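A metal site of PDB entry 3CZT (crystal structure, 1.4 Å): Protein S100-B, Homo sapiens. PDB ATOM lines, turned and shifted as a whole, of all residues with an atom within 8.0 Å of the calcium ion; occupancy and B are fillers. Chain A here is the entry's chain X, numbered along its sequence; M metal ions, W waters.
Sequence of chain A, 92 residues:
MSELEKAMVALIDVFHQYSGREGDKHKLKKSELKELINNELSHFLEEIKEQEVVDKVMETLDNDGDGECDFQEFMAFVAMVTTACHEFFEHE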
ATOM      1  N   PHE A  15      22.950  -9.190  23.612  1.00  0.00           N
ATOM      2  CA  PHE A  15      23.357  -9.061  22.204  1.00  0.00           C
ATOM      3  C   PHE A  15      24.229 -10.280  21.822  1.00  0.00           C
ATOM      4  O   PHE A  15      24.010 -10.952  20.824  1.00  0.00           O
ATOM      5  CB  PHE A  15      24.162  -7.791  21.954  1.00  0.00           C
ATOM      6  CG  PHE A  15      24.685  -7.676  20.554  1.00  0.00           C
ATOM      7  CD1 PHE A  15      23.858  -7.245  19.518  1.00  0.00           C
ATOM      8  CD2 PHE A  15      25.987  -8.095  20.248  1.00  0.00           C
ATOM      9  CE1 PHE A  15      24.357  -7.140  18.218  1.00  0.00           C
ATOM     10  CE2 PHE A  15      26.468  -7.959  18.955  1.00  0.00           C
ATOM     11  CZ  PHE A  15      25.691  -7.525  17.952  1.00  0.00           C
ATOM     12  N   HIS A  16      25.173 -10.603  22.658  1.00  0.00           N
ATOM     13  CA  HIS A  16      26.056 -11.782  22.393  1.00  0.00           C
ATOM     14  C   HIS A  16      25.280 -13.089  22.338  1.00  0.00           C
ATOM     15  O   HIS A  16      25.567 -13.970  21.521  1.00  0.00           O
ATOM     16  CB  HIS A  16      27.094 -11.923  23.495  1.00  0.00           C
ATOM     17  CG  HIS A  16      28.260 -11.006  23.375  1.00  0.00           C
ATOM     18  ND1 HIS A  16      29.028 -10.675  24.482  1.00  0.00           N
ATOM     19  CD2 HIS A  16      28.886 -10.476  22.308  1.00  0.00           C
ATOM     20  CE1 HIS A  16      30.030  -9.898  24.091  1.00  0.00           C
ATOM     21  NE2 HIS A  16      30.000  -9.794  22.767  1.00  0.00           N
ATOM     22  N   GLN A  17      24.372 -13.304  23.249  1.00  0.00           N
ATOM     23  CA  GLN A  17      23.539 -14.522  23.296  1.00  0.00           C
ATOM     24  C   GLN A  17      22.920 -14.768  21.978  1.00  0.00           C
ATOM     25  O   GLN A  17      22.936 -15.883  21.434  1.00  0.00           O
ATOM     26  CB  GLN A  17      22.455 -14.414  24.393  1.00  0.00           C
ATOM     27  CG  GLN A  17      22.995 -14.566  25.814  1.00  0.00           C
ATOM     28  CD  GLN A  17      22.038 -14.001  26.893  1.00  0.00           C
ATOM     29  OE1 GLN A  17      20.846 -13.795  26.674  1.00  0.00           O
ATOM     30  NE2 GLN A  17      22.608 -13.728  28.087  1.00  0.00           N
ATOM     31  N   TYR A  18      22.241 -13.731  21.476  1.00  0.00           N
ATOM     32  CA  TYR A  18      21.502 -13.879  20.256  1.00  0.00           C
ATOM     33  C   TYR A  18      22.368 -13.805  19.006  1.00  0.00           C
ATOM     34  O   TYR A  18      22.150 -14.587  18.042  1.00  0.00           O
ATOM     35  CB  TYR A  18      20.288 -12.930  20.197  1.00  0.00           C
ATOM     36  CG  TYR A  18      19.167 -13.432  21.093  1.00  0.00           C
ATOM     37  CD1 TYR A  18      19.161 -13.126  22.464  1.00  0.00           C
ATOM     38  CD2 TYR A  18      18.161 -14.254  20.578  1.00  0.00           C
ATOM     39  CE1 TYR A  18      18.209 -13.618  23.285  1.00  0.00           C
ATOM     40  CE2 TYR A  18      17.201 -14.742  21.400  1.00  0.00           C
ATOM     41  CZ  TYR A  18      17.248 -14.455  22.742  1.00  0.00           C
ATOM     42  OH  TYR A  18      16.214 -14.989  23.495  1.00  0.00           O
ATOM     43  N   SER A  19      23.344 -12.902  18.982  1.00  0.00           N
ATOM     44  CA  SER A  19      24.167 -12.744  17.796  1.00  0.00           C
ATOM     45  C   SER A  19      25.043 -13.986  17.510  1.00  0.00           C
ATOM     46  O   SER A  19      25.353 -14.314  16.345  1.00  0.00           O
ATOM     47  CB  SER A  19      25.078 -11.526  17.908  1.00  0.00           C
ATOM     48  OG  SER A  19      26.059 -11.644  18.931  1.00  0.00           O
ATOM     49  N   GLY A  20      25.383 -14.695  18.582  1.00  0.00           N
ATOM     50  CA  GLY A  20      26.247 -15.858  18.522  1.00  0.00           C
ATOM     51  C   GLY A  20      25.577 -17.115  17.978  1.00  0.00           C
ATOM     52  O   GLY A  20      26.255 -18.134  17.791  1.00  0.00           O
ATOM     53  N   ARG A  21      24.274 -17.088  17.677  1.00  0.00           N
ATOM     54  CA  ARG A  21      23.590 -18.330  17.300  1.00  0.00           C
ATOM     55  C   ARG A  21      24.004 -18.843  15.948  1.00  0.00           C
ATOM     56  O   ARG A  21      24.222 -20.046  15.781  1.00  0.00           O
ATOM     57  CB  ARG A  21      22.083 -18.164  17.384  1.00  0.00           C
ATOM     58  CG  ARG A  21      21.586 -17.916  18.796  1.00  0.00           C
ATOM     59  CD  ARG A  21      20.100 -17.731  18.823  1.00  0.00           C
ATOM     60  NE  ARG A  21      19.545 -17.722  20.157  1.00  0.00           N
ATOM     61  CZ  ARG A  21      18.252 -17.807  20.431  1.00  0.00           C
ATOM     62  NH1 ARG A  21      17.335 -17.939  19.453  1.00  0.00           N
ATOM     63  NH2 ARG A  21      17.857 -17.832  21.681  1.00  0.00           N
ATOM     64  N   GLU A  22      24.116 -17.957  14.974  1.00  0.00           N
ATOM     65  CA  GLU A  22      24.361 -18.339  13.588  1.00  0.00           C
ATOM     66  C   GLU A  22      25.198 -17.284  12.885  1.00  0.00           C
ATOM     67  O   GLU A  22      25.166 -16.091  13.235  1.00  0.00           O
ATOM     68  CB  GLU A  22      23.030 -18.458  12.824  1.00  0.00           C
ATOM     69  CG  GLU A  22      22.011 -19.458  13.388  1.00  0.00           C
ATOM     70  CD  GLU A  22      20.728 -19.565  12.541  1.00  0.00           C
ATOM     71  OE1 GLU A  22      19.657 -19.990  13.094  1.00  0.00           O
ATOM     72  OE2 GLU A  22      20.797 -19.211  11.323  1.00  0.00           O
ATOM     73  N   GLY A  23      25.951 -17.701  11.864  1.00  0.00           N
ATOM     74  CA  GLY A  23      26.612 -16.736  11.045  1.00  0.00           C
ATOM     75  C   GLY A  23      27.609 -15.941  11.811  1.00  0.00           C
ATOM     76  O   GLY A  23      28.287 -16.465  12.698  1.00  0.00           O
ATOM     77  N   ASP A  24      27.733 -14.679  11.422  1.00  0.00           N
ATOM     78  CA  ASP A  24      28.609 -13.718  12.075  1.00  0.00           C
ATOM     79  C   ASP A  24      28.186 -13.650  13.545  1.00  0.00           C
ATOM     80  O   ASP A  24      27.031 -13.346  13.843  1.00  0.00           O
ATOM     81  CB  ASP A  24      28.468 -12.346  11.413  1.00  0.00           C
ATOM     82  CG  ASP A  24      29.436 -11.326  11.913  1.00  0.00           C
ATOM     83  OD1 ASP A  24      29.797 -11.386  13.111  1.00  0.00           O
ATOM     84  OD2 ASP A  24      29.816 -10.437  11.119  1.00  0.00           O
ATOM     85  N   LYS A  25      29.111 -13.937  14.452  1.00  0.00           N
ATOM     86  CA  LYS A  25      28.754 -14.064  15.895  1.00  0.00           C
ATOM     87  C   LYS A  25      28.641 -12.688  16.594  1.00  0.00           C
ATOM     88  O   LYS A  25      28.370 -12.611  17.787  1.00  0.00           O
ATOM     89  CB  LYS A  25      29.733 -15.035  16.616  1.00  0.00           C
ATOM     90  CG  LYS A  25      29.503 -16.484  16.192  1.00  0.00           C
ATOM     91  CD  LYS A  25      30.118 -17.477  17.121  1.00  0.00           C
ATOM     92  CE  LYS A  25      29.720 -18.911  16.792  1.00  0.00           C
ATOM     93  NZ  LYS A  25      30.455 -19.819  17.690  1.00  0.00           N
ATOM     94  N   HIS A  26      28.881 -11.621  15.828  1.00  0.00           N
ATOM     95  CA  HIS A  26      28.751 -10.259  16.294  1.00  0.00           C
ATOM     96  C   HIS A  26      27.716  -9.488  15.548  1.00  0.00           C
ATOM     97  O   HIS A  26      27.679  -8.272  15.556  1.00  0.00           O
ATOM     98  CB  HIS A  26      30.067  -9.515  16.361  1.00  0.00           C
ATOM     99  CG  HIS A  26      30.704  -9.619  17.708  1.00  0.00           C
ATOM    100  ND1 HIS A  26      31.394 -10.746  18.088  1.00  0.00           N
ATOM    101  CD2 HIS A  26      30.637  -8.829  18.804  1.00  0.00           C
ATOM    102  CE1 HIS A  26      31.766 -10.597  19.348  1.00  0.00           C
ATOM    103  NE2 HIS A  26      31.287  -9.459  19.810  1.00  0.00           N
ATOM    104  N   LYS A  27      26.875 -10.215  14.817  1.00  0.00           N
ATOM    105  CA  LYS A  27      25.712  -9.582  14.212  1.00  0.00           C
ATOM    106  C   LYS A  27      24.470 -10.431  14.367  1.00  0.00           C
ATOM    107  O   LYS A  27      24.553 -11.613  14.426  1.00  0.00           O
ATOM    108  CB  LYS A  27      25.933  -9.275  12.739  1.00  0.00           C
ATOM    109  CG  LYS A  27      27.126  -8.393  12.365  1.00  0.00           C
ATOM    110  CD  LYS A  27      27.221  -8.160  10.845  1.00  0.00           C
ATOM    111  CE  LYS A  27      28.493  -7.364  10.437  1.00  0.00           C
ATOM    112  NZ  LYS A  27      28.580  -7.251   8.916  1.00  0.00           N
ATOM    113  N   LEU A  28      23.324  -9.753  14.449  1.00  0.00           N
ATOM    114  CA  LEU A  28      21.987 -10.391  14.453  1.00  0.00           C
ATOM    115  C   LEU A  28      21.410 -10.489  13.060  1.00  0.00           C
ATOM    116  O   LEU A  28      21.203  -9.483  12.414  1.00  0.00           O
ATOM    117  CB  LEU A  28      21.004  -9.592  15.323  1.00  0.00           C
ATOM    118  CG  LEU A  28      21.379  -9.398  16.787  1.00  0.00           C
ATOM    119  CD1 LEU A  28      20.549  -8.250  17.372  1.00  0.00           C
ATOM    120  CD2 LEU A  28      21.092 -10.654  17.561  1.00  0.00           C
ATOM    121  N   LYS A  29      21.226 -11.716  12.602  1.00  0.00           N
ATOM    122  CA  LYS A  29      20.480 -11.961  11.387  1.00  0.00           C
ATOM    123  C   LYS A  29      18.994 -11.850  11.719  1.00  0.00           C
ATOM    124  O   LYS A  29      18.608 -11.787  12.921  1.00  0.00           O
ATOM    125  CB  LYS A  29      20.761 -13.357  10.775  1.00  0.00           C
ATOM    126  CG  LYS A  29      20.118 -14.513  11.524  1.00  0.00           C
ATOM    127  CD  LYS A  29      20.784 -15.862  11.167  1.00  0.00           C
ATOM    128  CE  LYS A  29      20.734 -16.111   9.691  1.00  0.00           C
ATOM    129  NZ  LYS A  29      20.148 -17.432   9.313  1.00  0.00           N
ATOM    130  N   LYS A  30      18.153 -11.866  10.699  1.00  0.00           N
ATOM    131  CA  LYS A  30      16.700 -11.701  10.940  1.00  0.00           C
ATOM    132  C   LYS A  30      16.184 -12.731  11.970  1.00  0.00           C
ATOM    133  O   LYS A  30      15.408 -12.379  12.880  1.00  0.00           O
ATOM    134  CB  LYS A  30      15.908 -11.848   9.650  1.00  0.00           C
ATOM    135  CG  LYS A  30      15.889 -10.654   8.760  1.00  0.00           C
ATOM    136  CD  LYS A  30      15.037 -10.955   7.513  1.00  0.00           C
ATOM    137  CE  LYS A  30      14.944  -9.841   6.494  1.00  0.00           C
ATOM    138  NZ  LYS A  30      14.425 -10.430   5.210  1.00  0.00           N
ATOM    139  N   SER A  31      16.615 -13.973  11.884  1.00  0.00           N
ATOM    140  CA  SER A  31      16.053 -14.968  12.796  1.00  0.00           C
ATOM    141  C   SER A  31      16.444 -14.702  14.227  1.00  0.00           C
ATOM    142  O   SER A  31      15.624 -14.842  15.142  1.00  0.00           O
ATOM    143  CB  SER A  31      16.414 -16.383  12.416  1.00  0.00           C
ATOM    144  OG  SER A  31      17.769 -16.552  12.195  1.00  0.00           O
ATOM    145  N   GLU A  32      17.703 -14.298  14.379  1.00  0.00           N
ATOM    146  CA  GLU A  32      18.205 -13.995  15.706  1.00  0.00           C
ATOM    147  C   GLU A  32      17.510 -12.767  16.307  1.00  0.00           C
ATOM    148  O   GLU A  32      17.142 -12.735  17.502  1.00  0.00           O
ATOM    149  CB  GLU A  32      19.711 -13.748  15.677  1.00  0.00           C
ATOM    150  CG  GLU A  32      20.552 -14.977  15.259  1.00  0.00           C
ATOM    151  CD  GLU A  32      21.991 -14.653  14.916  1.00  0.00           C
ATOM    152  OE1 GLU A  32      22.301 -13.545  14.437  1.00  0.00           O
ATOM    153  OE2 GLU A  32      22.893 -15.525  15.090  1.00  0.00           O
ATOM    154  N   LEU A  33      17.331 -11.780  15.455  1.00  0.00           N
ATOM    155  CA  LEU A  33      16.623 -10.578  15.888  1.00  0.00           C
ATOM    156  C   LEU A  33      15.198 -10.864  16.297  1.00  0.00           C
ATOM    157  O   LEU A  33      14.689 -10.346  17.268  1.00  0.00           O
ATOM    158  CB  LEU A  33      16.671  -9.533  14.756  1.00  0.00           C
ATOM    159  CG  LEU A  33      15.950  -8.218  14.983  1.00  0.00           C
ATOM    160  CD1 LEU A  33      16.577  -7.412  16.128  1.00  0.00           C
ATOM    161  CD2 LEU A  33      15.840  -7.340  13.696  1.00  0.00           C
ATOM    162  N   GLU A  68      21.895  -7.230   8.426  1.00  0.00           N
ATOM    163  CA  GLU A  68      22.034  -7.691   9.813  1.00  0.00           C
ATOM    164  C   GLU A  68      22.113  -6.500  10.721  1.00  0.00           C
ATOM    165  O   GLU A  68      22.353  -5.362  10.288  1.00  0.00           O
ATOM    166  CB  GLU A  68      23.283  -8.561   9.958  1.00  0.00           C
ATOM    167  CG  GLU A  68      23.309  -9.754   9.015  1.00  0.00           C
ATOM    168  CD  GLU A  68      24.176 -10.881   9.486  1.00  0.00           C
ATOM    169  OE1 GLU A  68      24.130 -11.182  10.708  1.00  0.00           O
ATOM    170  OE2 GLU A  68      24.896 -11.454   8.633  1.00  0.00           O
ATOM    171  N   CYS A  69      21.914  -6.767  12.005  1.00  0.00           N
ATOM    172  CA  CYS A  69      22.060  -5.765  13.038  1.00  0.00           C
ATOM    173  C   CYS A  69      23.351  -5.991  13.776  1.00  0.00           C
ATOM    174  O   CYS A  69      23.490  -6.963  14.459  1.00  0.00           O
ATOM    175  CB  CYS A  69      20.864  -5.805  14.013  1.00  0.00           C
ATOM    176  SG  CYS A  69      20.859  -4.610  15.255  1.00  0.00           S
HETATM  177 CA    CA M   1      24.643 -13.966  14.123  1.00  0.00          CA
HETATM  178  O   HOH W   1      24.240 -13.439  11.903  1.00  0.00           O
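OG of Ser 19 sits at hydrogen-bond distance from O of Lys 25 (2.8 Å). OD1 of Asp 24 lies within hydrogen-bond range of N of His 26. OE2 of Glu 22 lies within salt-bridge range of NZ of Lys 29 (2.8 Å). The side-chain hydroxyl (OG) of Ser 19 is in hydrogen-bond range of the backbone carbonyl oxygen (O) of Phe 15 (2.9 Å). The side-chain carboxylate (OE2) of Glu 32 sits close to the backbone NH (N) of Arg 21 (3.3 Å). The backbone NH (N) of Lys 29 lies close to the side-chain carboxylate (OE1) of Glu 32 (2.8 Å).
Within 4 Å of the calcium ion: Ser 19, Glu 22, Asp 24, Lys 27 and Glu 32. Along chain A the residues within 4 Å of the calcium ion span positions 19 to 32.
The calcium ion is bound by water W1 (2.3 Å), O of Ser 19 (2.4 Å), O of Glu 22 (2.4 Å), O of Lys 27 (2.4 Å), OE1 of Glu 32 (2.4 Å), O of Asp 24 (2.5 Å) and OE2 of Glu 32 (2.5 Å). The calcium ion has seven donor atoms within binding distance.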
